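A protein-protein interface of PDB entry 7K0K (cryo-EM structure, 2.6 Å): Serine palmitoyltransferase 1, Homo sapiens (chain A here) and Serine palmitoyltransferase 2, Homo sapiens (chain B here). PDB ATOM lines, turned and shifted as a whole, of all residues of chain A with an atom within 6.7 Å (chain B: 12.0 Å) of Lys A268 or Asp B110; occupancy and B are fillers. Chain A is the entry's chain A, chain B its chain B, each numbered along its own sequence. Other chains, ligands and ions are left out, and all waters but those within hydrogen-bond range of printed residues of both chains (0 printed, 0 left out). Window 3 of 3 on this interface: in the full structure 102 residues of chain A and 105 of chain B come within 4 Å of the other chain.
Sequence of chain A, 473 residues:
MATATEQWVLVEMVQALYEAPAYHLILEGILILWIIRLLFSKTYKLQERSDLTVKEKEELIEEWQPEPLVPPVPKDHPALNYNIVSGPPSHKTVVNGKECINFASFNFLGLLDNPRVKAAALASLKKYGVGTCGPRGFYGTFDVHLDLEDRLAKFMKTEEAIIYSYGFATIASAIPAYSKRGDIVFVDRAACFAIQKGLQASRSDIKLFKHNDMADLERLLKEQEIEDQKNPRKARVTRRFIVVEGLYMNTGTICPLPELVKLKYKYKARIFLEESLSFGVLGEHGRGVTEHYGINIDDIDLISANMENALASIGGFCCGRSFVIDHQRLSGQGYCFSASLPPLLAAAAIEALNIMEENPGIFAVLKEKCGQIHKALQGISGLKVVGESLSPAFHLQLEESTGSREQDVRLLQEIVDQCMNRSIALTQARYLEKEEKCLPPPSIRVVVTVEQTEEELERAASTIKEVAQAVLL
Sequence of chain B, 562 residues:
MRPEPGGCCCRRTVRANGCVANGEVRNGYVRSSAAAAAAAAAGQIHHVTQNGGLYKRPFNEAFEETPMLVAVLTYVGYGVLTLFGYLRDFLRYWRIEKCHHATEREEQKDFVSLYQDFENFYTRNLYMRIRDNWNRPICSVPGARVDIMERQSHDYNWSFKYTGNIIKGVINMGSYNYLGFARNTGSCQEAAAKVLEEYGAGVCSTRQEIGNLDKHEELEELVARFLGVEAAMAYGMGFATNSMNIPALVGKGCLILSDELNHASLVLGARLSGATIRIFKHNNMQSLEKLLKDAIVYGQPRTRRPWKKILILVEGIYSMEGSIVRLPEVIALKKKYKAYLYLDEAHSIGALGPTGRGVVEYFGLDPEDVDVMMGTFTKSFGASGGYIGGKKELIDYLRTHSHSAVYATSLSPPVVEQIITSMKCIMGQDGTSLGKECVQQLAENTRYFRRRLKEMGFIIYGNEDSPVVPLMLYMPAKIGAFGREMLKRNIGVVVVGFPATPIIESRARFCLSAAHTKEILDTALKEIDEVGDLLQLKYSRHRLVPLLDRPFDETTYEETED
The guanidinium group (NH1) of Arg A239 lies close to the backbone carbonyl oxygen (O) of Leu B114 (3.3 Å). OE1 of Gln B116 is in hydrogen-bond range of NH1 of Arg A239 (2.9 Å). OE1 of Gln B108 sits at hydrogen-bond distance from NZ of Lys A264, 2.9 Å away. The guanidinium group (NH1) of Arg B105 lies within hydrogen-bond range of the side-chain hydroxyl (OH) of Tyr A265. The side-chain carboxylate (OE1) of Glu B104 lies within salt-bridge range of the guanidinium group (NH1) of Arg A270, 3.2 Å away. NH2 of Arg A270 sits at hydrogen-bond distance from O of Val B112 (2.8 Å). The backbone NH (N) of Leu B114 lies close to the guanidinium group (NH1) of Arg A270.
Of chain B, only Asp B110 and Phe B111 come within 4 Å of Lys A268. Asp B110 touches just one residue of chain A: Lys A268 (3.7 Å). Arg A240 touches one residue of chain B. Ala A269 touches none of the printed residues of chain B. Of the printed residues of chain B, Lys A264 touches Gln B108 (2.9 Å) and Phe B111 (3.9 Å). Printed residues of chain A within 4 Å of Gln B116: Arg A239. Tyr A267 touches none of the printed residues of chain B. The nearest printed residue of chain A that does not touch Asp B110 is Arg A270 (6.7 Å). The nearest printed residue of chain B that does not touch Arg A270 is Ser B113 (4.02 Å).
The backbone carbonyl oxygen (O) of Thr A238 sits at hydrogen-bond distance from the guanidinium group (NH1) of Arg A240, 2.5 Å away. The backbone carbonyl oxygen (O) of Lys A264 lies within hydrogen-bond range of the backbone NH (N) of Ala A269 (3.3 Å). NE2 of Gln B108 lies within hydrogen-bond range of OE2 of Glu B104 (3.3 Å). The guanidinium group of Arg B105 lies within salt-bridge range of the side-chain carboxylate of Glu B107, at 3.4 Å. The guanidinium group (NH1) of Arg B105 sits at hydrogen-bond distance from the side-chain amide oxygen (OE1) of Gln B108, 3.1 Å away. The backbone carbonyl oxygen (O) of Tyr B115 sits at hydrogen-bond distance from the side-chain hydroxyl (OG) of Ser B113, 3.5 Å away.
Hydrophobic or aromatic side chains of chain A within 4 Å of the printed part of chain B: Tyr A265. Of the 14 printed residues of chain B, 9 touch a printed residue of chain A. Printed residues of chain B that touch a printed residue of chain A: Glu B104, Arg B105, Gln B108, Asp B110, Phe B111, Val B112, Ser B113, Leu B114 and Gln B116. Hydrophobic or aromatic side chains of chain B that line the printed part of chain A: Phe B111, Val B112 and Leu B114. Among the printed residues, 17 pairs touch across the chains.
Among the printed residues, pairs that only touch across the chains: Thr A238 with Val B112, Arg A239 with Ser B113, Lys A268 with Phe B111, Arg A239 with Val B112, Arg A270 with Phe B111, Arg A240 with Val B112, Lys A268 with Asp B110, Arg A270 with Gln B108, Lys A264 with Phe B111 and Tyr A265 with Phe B111.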
ATOM      1  N   LEU A 221      16.973  12.802 -29.866  1.00  0.00           N
ATOM      2  CA  LEU A 221      18.416  12.768 -30.071  1.00  0.00           C
ATOM      3  C   LEU A 221      18.778  12.231 -31.451  1.00  0.00           C
ATOM      4  O   LEU A 221      19.684  12.754 -32.103  1.00  0.00           O
ATOM      5  CB  LEU A 221      19.069  11.935 -28.974  1.00  0.00           C
ATOM      6  CG  LEU A 221      19.076  12.615 -27.608  1.00  0.00           C
ATOM      7  CD1 LEU A 221      19.413  11.617 -26.520  1.00  0.00           C
ATOM      8  CD2 LEU A 221      20.054  13.772 -27.600  1.00  0.00           C
ATOM      9  N   THR A 238      27.971  23.092 -32.147  1.00  0.00           N
ATOM     10  CA  THR A 238      26.699  23.082 -31.439  1.00  0.00           C
ATOM     11  C   THR A 238      26.795  22.188 -30.211  1.00  0.00           C
ATOM     12  O   THR A 238      27.181  21.020 -30.317  1.00  0.00           O
ATOM     13  CB  THR A 238      25.578  22.596 -32.357  1.00  0.00           C
ATOM     14  OG1 THR A 238      25.229  23.635 -33.276  1.00  0.00           O
ATOM     15  CG2 THR A 238      24.351  22.216 -31.553  1.00  0.00           C
ATOM     16  N   ARG A 239      26.438  22.734 -29.054  1.00  0.00           N
ATOM     17  CA  ARG A 239      26.495  22.010 -27.794  1.00  0.00           C
ATOM     18  C   ARG A 239      25.126  21.458 -27.437  1.00  0.00           C
ATOM     19  O   ARG A 239      24.100  22.083 -27.717  1.00  0.00           O
ATOM     20  CB  ARG A 239      26.996  22.913 -26.672  1.00  0.00           C
ATOM     21  CG  ARG A 239      28.478  23.152 -26.714  1.00  0.00           C
ATOM     22  CD  ARG A 239      28.932  23.942 -25.521  1.00  0.00           C
ATOM     23  NE  ARG A 239      28.331  25.267 -25.496  1.00  0.00           N
ATOM     24  CZ  ARG A 239      28.895  26.349 -26.016  1.00  0.00           C
ATOM     25  NH1 ARG A 239      30.074  26.256 -26.609  1.00  0.00           N
ATOM     26  NH2 ARG A 239      28.281  27.519 -25.946  1.00  0.00           N
ATOM     27  N   ARG A 240      25.115  20.283 -26.820  1.00  0.00           N
ATOM     28  CA  ARG A 240      23.889  19.588 -26.468  1.00  0.00           C
ATOM     29  C   ARG A 240      23.832  19.391 -24.963  1.00  0.00           C
ATOM     30  O   ARG A 240      24.793  18.903 -24.361  1.00  0.00           O
ATOM     31  CB  ARG A 240      23.803  18.242 -27.180  1.00  0.00           C
ATOM     32  CG  ARG A 240      23.682  18.345 -28.683  1.00  0.00           C
ATOM     33  CD  ARG A 240      24.370  17.174 -29.352  1.00  0.00           C
ATOM     34  NE  ARG A 240      24.585  17.396 -30.776  1.00  0.00           N
ATOM     35  CZ  ARG A 240      25.588  18.106 -31.274  1.00  0.00           C
ATOM     36  NH1 ARG A 240      26.468  18.667 -30.460  1.00  0.00           N
ATOM     37  NH2 ARG A 240      25.709  18.256 -32.584  1.00  0.00           N
ATOM     38  N   PHE A 241      22.710  19.774 -24.363  1.00  0.00           N
ATOM     39  CA  PHE A 241      22.490  19.627 -22.934  1.00  0.00           C
ATOM     40  C   PHE A 241      21.202  18.858 -22.710  1.00  0.00           C
ATOM     41  O   PHE A 241      20.207  19.095 -23.397  1.00  0.00           O
ATOM     42  CB  PHE A 241      22.409  20.984 -22.233  1.00  0.00           C
ATOM     43  CG  PHE A 241      23.635  21.827 -22.394  1.00  0.00           C
ATOM     44  CD1 PHE A 241      24.690  21.715 -21.512  1.00  0.00           C
ATOM     45  CD2 PHE A 241      23.731  22.737 -23.426  1.00  0.00           C
ATOM     46  CE1 PHE A 241      25.813  22.491 -21.660  1.00  0.00           C
ATOM     47  CE2 PHE A 241      24.853  23.511 -23.575  1.00  0.00           C
ATOM     48  CZ  PHE A 241      25.894  23.387 -22.693  1.00  0.00           C
ATOM     49  N   LYS A 262      23.558   6.621 -20.161  1.00  0.00           N
ATOM     50  CA  LYS A 262      23.846   5.897 -21.394  1.00  0.00           C
ATOM     51  C   LYS A 262      23.546   6.749 -22.623  1.00  0.00           C
ATOM     52  O   LYS A 262      24.331   6.774 -23.578  1.00  0.00           O
ATOM     53  CB  LYS A 262      23.056   4.592 -21.430  1.00  0.00           C
ATOM     54  CG  LYS A 262      23.501   3.602 -20.387  1.00  0.00           C
ATOM     55  CD  LYS A 262      23.227   2.184 -20.815  1.00  0.00           C
ATOM     56  CE  LYS A 262      24.172   1.217 -20.127  1.00  0.00           C
ATOM     57  NZ  LYS A 262      24.818   0.288 -21.095  1.00  0.00           N
ATOM     58  N   LEU A 263      22.420   7.467 -22.613  1.00  0.00           N
ATOM     59  CA  LEU A 263      22.081   8.332 -23.736  1.00  0.00           C
ATOM     60  C   LEU A 263      23.049   9.499 -23.846  1.00  0.00           C
ATOM     61  O   LEU A 263      23.369   9.949 -24.950  1.00  0.00           O
ATOM     62  CB  LEU A 263      20.649   8.841 -23.594  1.00  0.00           C
ATOM     63  CG  LEU A 263      19.547   7.904 -24.075  1.00  0.00           C
ATOM     64  CD1 LEU A 263      18.202   8.405 -23.608  1.00  0.00           C
ATOM     65  CD2 LEU A 263      19.569   7.775 -25.576  1.00  0.00           C
ATOM     66  N   LYS A 264      23.511  10.014 -22.707  1.00  0.00           N
ATOM     67  CA  LYS A 264      24.514  11.069 -22.712  1.00  0.00           C
ATOM     68  C   LYS A 264      25.776  10.622 -23.420  1.00  0.00           C
ATOM     69  O   LYS A 264      26.342  11.368 -24.223  1.00  0.00           O
ATOM     70  CB  LYS A 264      24.845  11.488 -21.281  1.00  0.00           C
ATOM     71  CG  LYS A 264      26.201  12.149 -21.150  1.00  0.00           C
ATOM     72  CD  LYS A 264      26.507  12.559 -19.732  1.00  0.00           C
ATOM     73  CE  LYS A 264      27.918  13.083 -19.633  1.00  0.00           C
ATOM     74  NZ  LYS A 264      28.234  13.568 -18.271  1.00  0.00           N
ATOM     75  N   TYR A 265      26.242   9.415 -23.129  1.00  0.00           N
ATOM     76  CA  TYR A 265      27.476   8.979 -23.770  1.00  0.00           C
ATOM     77  C   TYR A 265      27.256   8.552 -25.214  1.00  0.00           C
ATOM     78  O   TYR A 265      28.181   8.647 -26.028  1.00  0.00           O
ATOM     79  CB  TYR A 265      28.133   7.876 -22.949  1.00  0.00           C
ATOM     80  CG  TYR A 265      28.809   8.445 -21.732  1.00  0.00           C
ATOM     81  CD1 TYR A 265      29.774   9.431 -21.859  1.00  0.00           C
ATOM     82  CD2 TYR A 265      28.463   8.028 -20.459  1.00  0.00           C
ATOM     83  CE1 TYR A 265      30.388   9.970 -20.759  1.00  0.00           C
ATOM     84  CE2 TYR A 265      29.074   8.562 -19.348  1.00  0.00           C
ATOM     85  CZ  TYR A 265      30.037   9.533 -19.505  1.00  0.00           C
ATOM     86  OH  TYR A 265      30.653  10.070 -18.401  1.00  0.00           O
ATOM     87  N   LYS A 266      26.053   8.093 -25.563  1.00  0.00           N
ATOM     88  CA  LYS A 266      25.804   7.710 -26.949  1.00  0.00           C
ATOM     89  C   LYS A 266      25.644   8.928 -27.855  1.00  0.00           C
ATOM     90  O   LYS A 266      26.146   8.935 -28.984  1.00  0.00           O
ATOM     91  CB  LYS A 266      24.578   6.805 -27.037  1.00  0.00           C
ATOM     92  CG  LYS A 266      24.202   6.438 -28.458  1.00  0.00           C
ATOM     93  CD  LYS A 266      22.983   5.544 -28.520  1.00  0.00           C
ATOM     94  CE  LYS A 266      23.351   4.084 -28.460  1.00  0.00           C
ATOM     95  NZ  LYS A 266      23.949   3.635 -29.744  1.00  0.00           N
ATOM     96  N   TYR A 267      24.949   9.965 -27.390  1.00  0.00           N
ATOM     97  CA  TYR A 267      24.657  11.127 -28.220  1.00  0.00           C
ATOM     98  C   TYR A 267      25.397  12.376 -27.774  1.00  0.00           C
ATOM     99  O   TYR A 267      25.166  13.451 -28.334  1.00  0.00           O
ATOM    100  CB  TYR A 267      23.152  11.388 -28.258  1.00  0.00           C
ATOM    101  CG  TYR A 267      22.391  10.268 -28.916  1.00  0.00           C
ATOM    102  CD1 TYR A 267      22.373  10.137 -30.290  1.00  0.00           C
ATOM    103  CD2 TYR A 267      21.710   9.335 -28.163  1.00  0.00           C
ATOM    104  CE1 TYR A 267      21.694   9.115 -30.894  1.00  0.00           C
ATOM    105  CE2 TYR A 267      21.026   8.314 -28.759  1.00  0.00           C
ATOM    106  CZ  TYR A 267      21.024   8.205 -30.124  1.00  0.00           C
ATOM    107  OH  TYR A 267      20.339   7.176 -30.718  1.00  0.00           O
ATOM    108  N   LYS A 268      26.269  12.260 -26.779  1.00  0.00           N
ATOM    109  CA  LYS A 268      27.256  13.287 -26.463  1.00  0.00           C
ATOM    110  C   LYS A 268      26.597  14.595 -26.034  1.00  0.00           C
ATOM    111  O   LYS A 268      26.854  15.664 -26.589  1.00  0.00           O
ATOM    112  CB  LYS A 268      28.194  13.491 -27.646  1.00  0.00           C
ATOM    113  CG  LYS A 268      28.923  12.216 -28.008  1.00  0.00           C
ATOM    114  CD  LYS A 268      29.878  12.404 -29.154  1.00  0.00           C
ATOM    115  CE  LYS A 268      30.587  11.103 -29.459  1.00  0.00           C
ATOM    116  NZ  LYS A 268      31.518  10.720 -28.364  1.00  0.00           N
ATOM    117  N   ALA A 269      25.751  14.501 -25.011  1.00  0.00           N
ATOM    118  CA  ALA A 269      25.032  15.641 -24.462  1.00  0.00           C
ATOM    119  C   ALA A 269      25.281  15.719 -22.964  1.00  0.00           C
ATOM    120  O   ALA A 269      25.026  14.753 -22.242  1.00  0.00           O
ATOM    121  CB  ALA A 269      23.535  15.527 -24.747  1.00  0.00           C
ATOM    122  N   ARG A 270      25.759  16.869 -22.497  1.00  0.00           N
ATOM    123  CA  ARG A 270      26.097  17.031 -21.091  1.00  0.00           C
ATOM    124  C   ARG A 270      24.841  17.131 -20.234  1.00  0.00           C
ATOM    125  O   ARG A 270      23.838  17.711 -20.640  1.00  0.00           O
ATOM    126  CB  ARG A 270      26.957  18.276 -20.901  1.00  0.00           C
ATOM    127  CG  ARG A 270      28.298  18.170 -21.573  1.00  0.00           C
ATOM    128  CD  ARG A 270      29.159  19.371 -21.294  1.00  0.00           C
ATOM    129  NE  ARG A 270      30.499  19.191 -21.835  1.00  0.00           N
ATOM    130  CZ  ARG A 270      30.813  19.361 -23.113  1.00  0.00           C
ATOM    131  NH1 ARG A 270      32.059  19.177 -23.518  1.00  0.00           N
ATOM    132  NH2 ARG A 270      29.881  19.712 -23.984  1.00  0.00           N
ATOM    133  N   THR B 103      40.819  20.892 -17.377  1.00  0.00           N
ATOM    134  CA  THR B 103      40.500  20.424 -18.715  1.00  0.00           C
ATOM    135  C   THR B 103      39.325  19.460 -18.655  1.00  0.00           C
ATOM    136  O   THR B 103      39.029  18.872 -17.615  1.00  0.00           O
ATOM    137  CB  THR B 103      41.701  19.734 -19.378  1.00  0.00           C
ATOM    138  OG1 THR B 103      41.967  18.493 -18.713  1.00  0.00           O
ATOM    139  CG2 THR B 103      42.934  20.614 -19.308  1.00  0.00           C
ATOM    140  N   GLU B 104      38.649  19.317 -19.791  1.00  0.00           N
ATOM    141  CA  GLU B 104      37.570  18.351 -19.898  1.00  0.00           C
ATOM    142  C   GLU B 104      38.102  16.944 -19.664  1.00  0.00           C
ATOM    143  O   GLU B 104      39.232  16.614 -20.031  1.00  0.00           O
ATOM    144  CB  GLU B 104      36.906  18.450 -21.271  1.00  0.00           C
ATOM    145  CG  GLU B 104      35.693  17.550 -21.457  1.00  0.00           C
ATOM    146  CD  GLU B 104      34.544  17.902 -20.538  1.00  0.00           C
ATOM    147  OE1 GLU B 104      33.757  18.806 -20.883  1.00  0.00           O
ATOM    148  OE2 GLU B 104      34.423  17.272 -19.469  1.00  0.00           O
ATOM    149  N   ARG B 105      37.280  16.114 -19.032  1.00  0.00           N
ATOM    150  CA  ARG B 105      37.703  14.765 -18.694  1.00  0.00           C
ATOM    151  C   ARG B 105      37.885  13.919 -19.949  1.00  0.00           C
ATOM    152  O   ARG B 105      37.313  14.200 -21.004  1.00  0.00           O
ATOM    153  CB  ARG B 105      36.699  14.124 -17.738  1.00  0.00           C
ATOM    154  CG  ARG B 105      35.251  14.234 -18.164  1.00  0.00           C
ATOM    155  CD  ARG B 105      34.332  14.047 -16.974  1.00  0.00           C
ATOM    156  NE  ARG B 105      34.375  12.686 -16.457  1.00  0.00           N
ATOM    157  CZ  ARG B 105      33.507  11.734 -16.781  1.00  0.00           C
ATOM    158  NH1 ARG B 105      32.517  11.992 -17.619  1.00  0.00           N
ATOM    159  NH2 ARG B 105      33.629  10.524 -16.261  1.00  0.00           N
ATOM    160  N   GLU B 106      38.717  12.882 -19.829  1.00  0.00           N
ATOM    161  CA  GLU B 106      39.080  12.078 -20.991  1.00  0.00           C
ATOM    162  C   GLU B 106      37.869  11.378 -21.586  1.00  0.00           C
ATOM    163  O   GLU B 106      37.799  11.172 -22.803  1.00  0.00           O
ATOM    164  CB  GLU B 106      40.148  11.052 -20.611  1.00  0.00           C
ATOM    165  CG  GLU B 106      41.451  11.650 -20.112  1.00  0.00           C
ATOM    166  CD  GLU B 106      41.506  11.764 -18.601  1.00  0.00           C
ATOM    167  OE1 GLU B 106      40.540  11.341 -17.934  1.00  0.00           O
ATOM    168  OE2 GLU B 106      42.518  12.273 -18.079  1.00  0.00           O
ATOM    169  N   GLU B 107      36.912  10.990 -20.743  1.00  0.00           N
ATOM    170  CA  GLU B 107      35.726  10.301 -21.237  1.00  0.00           C
ATOM    171  C   GLU B 107      34.873  11.223 -22.098  1.00  0.00           C
ATOM    172  O   GLU B 107      34.109  10.758 -22.951  1.00  0.00           O
ATOM    173  CB  GLU B 107      34.912   9.757 -20.065  1.00  0.00           C
ATOM    174  CG  GLU B 107      35.618   8.679 -19.257  1.00  0.00           C
ATOM    175  CD  GLU B 107      36.588   9.245 -18.236  1.00  0.00           C
ATOM    176  OE1 GLU B 107      36.580  10.473 -18.020  1.00  0.00           O
ATOM    177  OE2 GLU B 107      37.362   8.460 -17.651  1.00  0.00           O
ATOM    178  N   GLN B 108      34.997  12.533 -21.898  1.00  0.00           N
ATOM    179  CA  GLN B 108      34.194  13.521 -22.598  1.00  0.00           C
ATOM    180  C   GLN B 108      35.017  14.391 -23.538  1.00  0.00           C
ATOM    181  O   GLN B 108      34.634  15.534 -23.802  1.00  0.00           O
ATOM    182  CB  GLN B 108      33.459  14.399 -21.588  1.00  0.00           C
ATOM    183  CG  GLN B 108      32.407  13.674 -20.788  1.00  0.00           C
ATOM    184  CD  GLN B 108      31.551  14.619 -19.986  1.00  0.00           C
ATOM    185  OE1 GLN B 108      30.917  14.222 -19.012  1.00  0.00           O
ATOM    186  NE2 GLN B 108      31.530  15.881 -20.384  1.00  0.00           N
ATOM    187  N   LYS B 109      36.144  13.886 -24.040  1.00  0.00           N
ATOM    188  CA  LYS B 109      36.978  14.705 -24.912  1.00  0.00           C
ATOM    189  C   LYS B 109      36.408  14.789 -26.319  1.00  0.00           C
ATOM    190  O   LYS B 109      36.719  15.733 -27.056  1.00  0.00           O
ATOM    191  CB  LYS B 109      38.403  14.161 -24.960  1.00  0.00           C
ATOM    192  CG  LYS B 109      38.526  12.784 -25.570  1.00  0.00           C
ATOM    193  CD  LYS B 109      39.961  12.304 -25.524  1.00  0.00           C
ATOM    194  CE  LYS B 109      40.108  10.936 -26.154  1.00  0.00           C
ATOM    195  NZ  LYS B 109      39.414   9.891 -25.354  1.00  0.00           N
ATOM    196  N   ASP B 110      35.582  13.826 -26.710  1.00  0.00           N
ATOM    197  CA  ASP B 110      34.982  13.822 -28.034  1.00  0.00           C
ATOM    198  C   ASP B 110      33.667  14.580 -28.092  1.00  0.00           C
ATOM    199  O   ASP B 110      33.010  14.561 -29.136  1.00  0.00           O
ATOM    200  CB  ASP B 110      34.771  12.387 -28.516  1.00  0.00           C
ATOM    201  CG  ASP B 110      36.053  11.744 -28.994  1.00  0.00           C
ATOM    202  OD1 ASP B 110      37.111  12.399 -28.906  1.00  0.00           O
ATOM    203  OD2 ASP B 110      36.005  10.590 -29.467  1.00  0.00           O
ATOM    204  N   PHE B 111      33.254  15.227 -27.007  1.00  0.00           N
ATOM    205  CA  PHE B 111      32.065  16.052 -27.090  1.00  0.00           C
ATOM    206  C   PHE B 111      32.421  17.388 -27.731  1.00  0.00           C
ATOM    207  O   PHE B 111      33.592  17.758 -27.840  1.00  0.00           O
ATOM    208  CB  PHE B 111      31.446  16.322 -25.716  1.00  0.00           C
ATOM    209  CG  PHE B 111      30.941  15.097 -25.005  1.00  0.00           C
ATOM    210  CD1 PHE B 111      30.897  13.872 -25.630  1.00  0.00           C
ATOM    211  CD2 PHE B 111      30.400  15.207 -23.744  1.00  0.00           C
ATOM    212  CE1 PHE B 111      30.417  12.764 -24.969  1.00  0.00           C
ATOM    213  CE2 PHE B 111      29.898  14.105 -23.095  1.00  0.00           C
ATOM    214  CZ  PHE B 111      29.906  12.885 -23.708  1.00  0.00           C
ATOM    215  N   VAL B 112      31.394  18.119 -28.162  1.00  0.00           N
ATOM    216  CA  VAL B 112      31.612  19.504 -28.547  1.00  0.00           C
ATOM    217  C   VAL B 112      32.071  20.272 -27.319  1.00  0.00           C
ATOM    218  O   VAL B 112      31.455  20.194 -26.250  1.00  0.00           O
ATOM    219  CB  VAL B 112      30.338  20.113 -29.152  1.00  0.00           C
ATOM    220  CG1 VAL B 112      30.494  21.606 -29.318  1.00  0.00           C
ATOM    221  CG2 VAL B 112      30.035  19.464 -30.484  1.00  0.00           C
ATOM    222  N   SER B 113      33.169  21.010 -27.465  1.00  0.00           N
ATOM    223  CA  SER B 113      33.818  21.621 -26.314  1.00  0.00           C
ATOM    224  C   SER B 113      32.856  22.537 -25.572  1.00  0.00           C
ATOM    225  O   SER B 113      32.090  23.288 -26.177  1.00  0.00           O
ATOM    226  CB  SER B 113      35.053  22.397 -26.758  1.00  0.00           C
ATOM    227  OG  SER B 113      34.706  23.441 -27.647  1.00  0.00           O
ATOM    228  N   LEU B 114      32.895  22.454 -24.242  1.00  0.00           N
ATOM    229  CA  LEU B 114      31.937  23.179 -23.416  1.00  0.00           C
ATOM    230  C   LEU B 114      32.076  24.683 -23.587  1.00  0.00           C
ATOM    231  O   LEU B 114      31.077  25.407 -23.610  1.00  0.00           O
ATOM    232  CB  LEU B 114      32.118  22.785 -21.953  1.00  0.00           C
ATOM    233  CG  LEU B 114      31.165  23.411 -20.943  1.00  0.00           C
ATOM    234  CD1 LEU B 114      29.733  23.264 -21.409  1.00  0.00           C
ATOM    235  CD2 LEU B 114      31.356  22.775 -19.584  1.00  0.00           C
ATOM    236  N   TYR B 115      33.305  25.174 -23.696  1.00  0.00           N
ATOM    237  CA  TYR B 115      33.569  26.595 -23.853  1.00  0.00           C
ATOM    238  C   TYR B 115      34.278  26.836 -25.173  1.00  0.00           C
ATOM    239  O   TYR B 115      35.224  26.120 -25.514  1.00  0.00           O
ATOM    240  CB  TYR B 115      34.423  27.132 -22.705  1.00  0.00           C
ATOM    241  CG  TYR B 115      34.019  26.623 -21.347  1.00  0.00           C
ATOM    242  CD1 TYR B 115      32.804  26.975 -20.789  1.00  0.00           C
ATOM    243  CD2 TYR B 115      34.851  25.789 -20.627  1.00  0.00           C
ATOM    244  CE1 TYR B 115      32.433  26.512 -19.553  1.00  0.00           C
ATOM    245  CE2 TYR B 115      34.489  25.324 -19.392  1.00  0.00           C
ATOM    246  CZ  TYR B 115      33.280  25.686 -18.860  1.00  0.00           C
ATOM    247  OH  TYR B 115      32.918  25.219 -17.623  1.00  0.00           O
ATOM    248  N   GLN B 116      33.812  27.832 -25.916  1.00  0.00           N
ATOM    249  CA  GLN B 116      34.592  28.349 -27.028  1.00  0.00           C
ATOM    250  C   GLN B 116      35.767  29.144 -26.475  1.00  0.00           C
ATOM    251  O   GLN B 116      35.606  29.963 -25.566  1.00  0.00           O
ATOM    252  CB  GLN B 116      33.722  29.220 -27.928  1.00  0.00           C
ATOM    253  CG  GLN B 116      32.398  28.575 -28.321  1.00  0.00           C
ATOM    254  CD  GLN B 116      32.576  27.278 -29.089  1.00  0.00           C
ATOM    255  OE1 GLN B 116      32.015  26.244 -28.725  1.00  0.00           O
ATOM    256  NE2 GLN B 116      33.348  27.330 -30.167  1.00  0.00           N
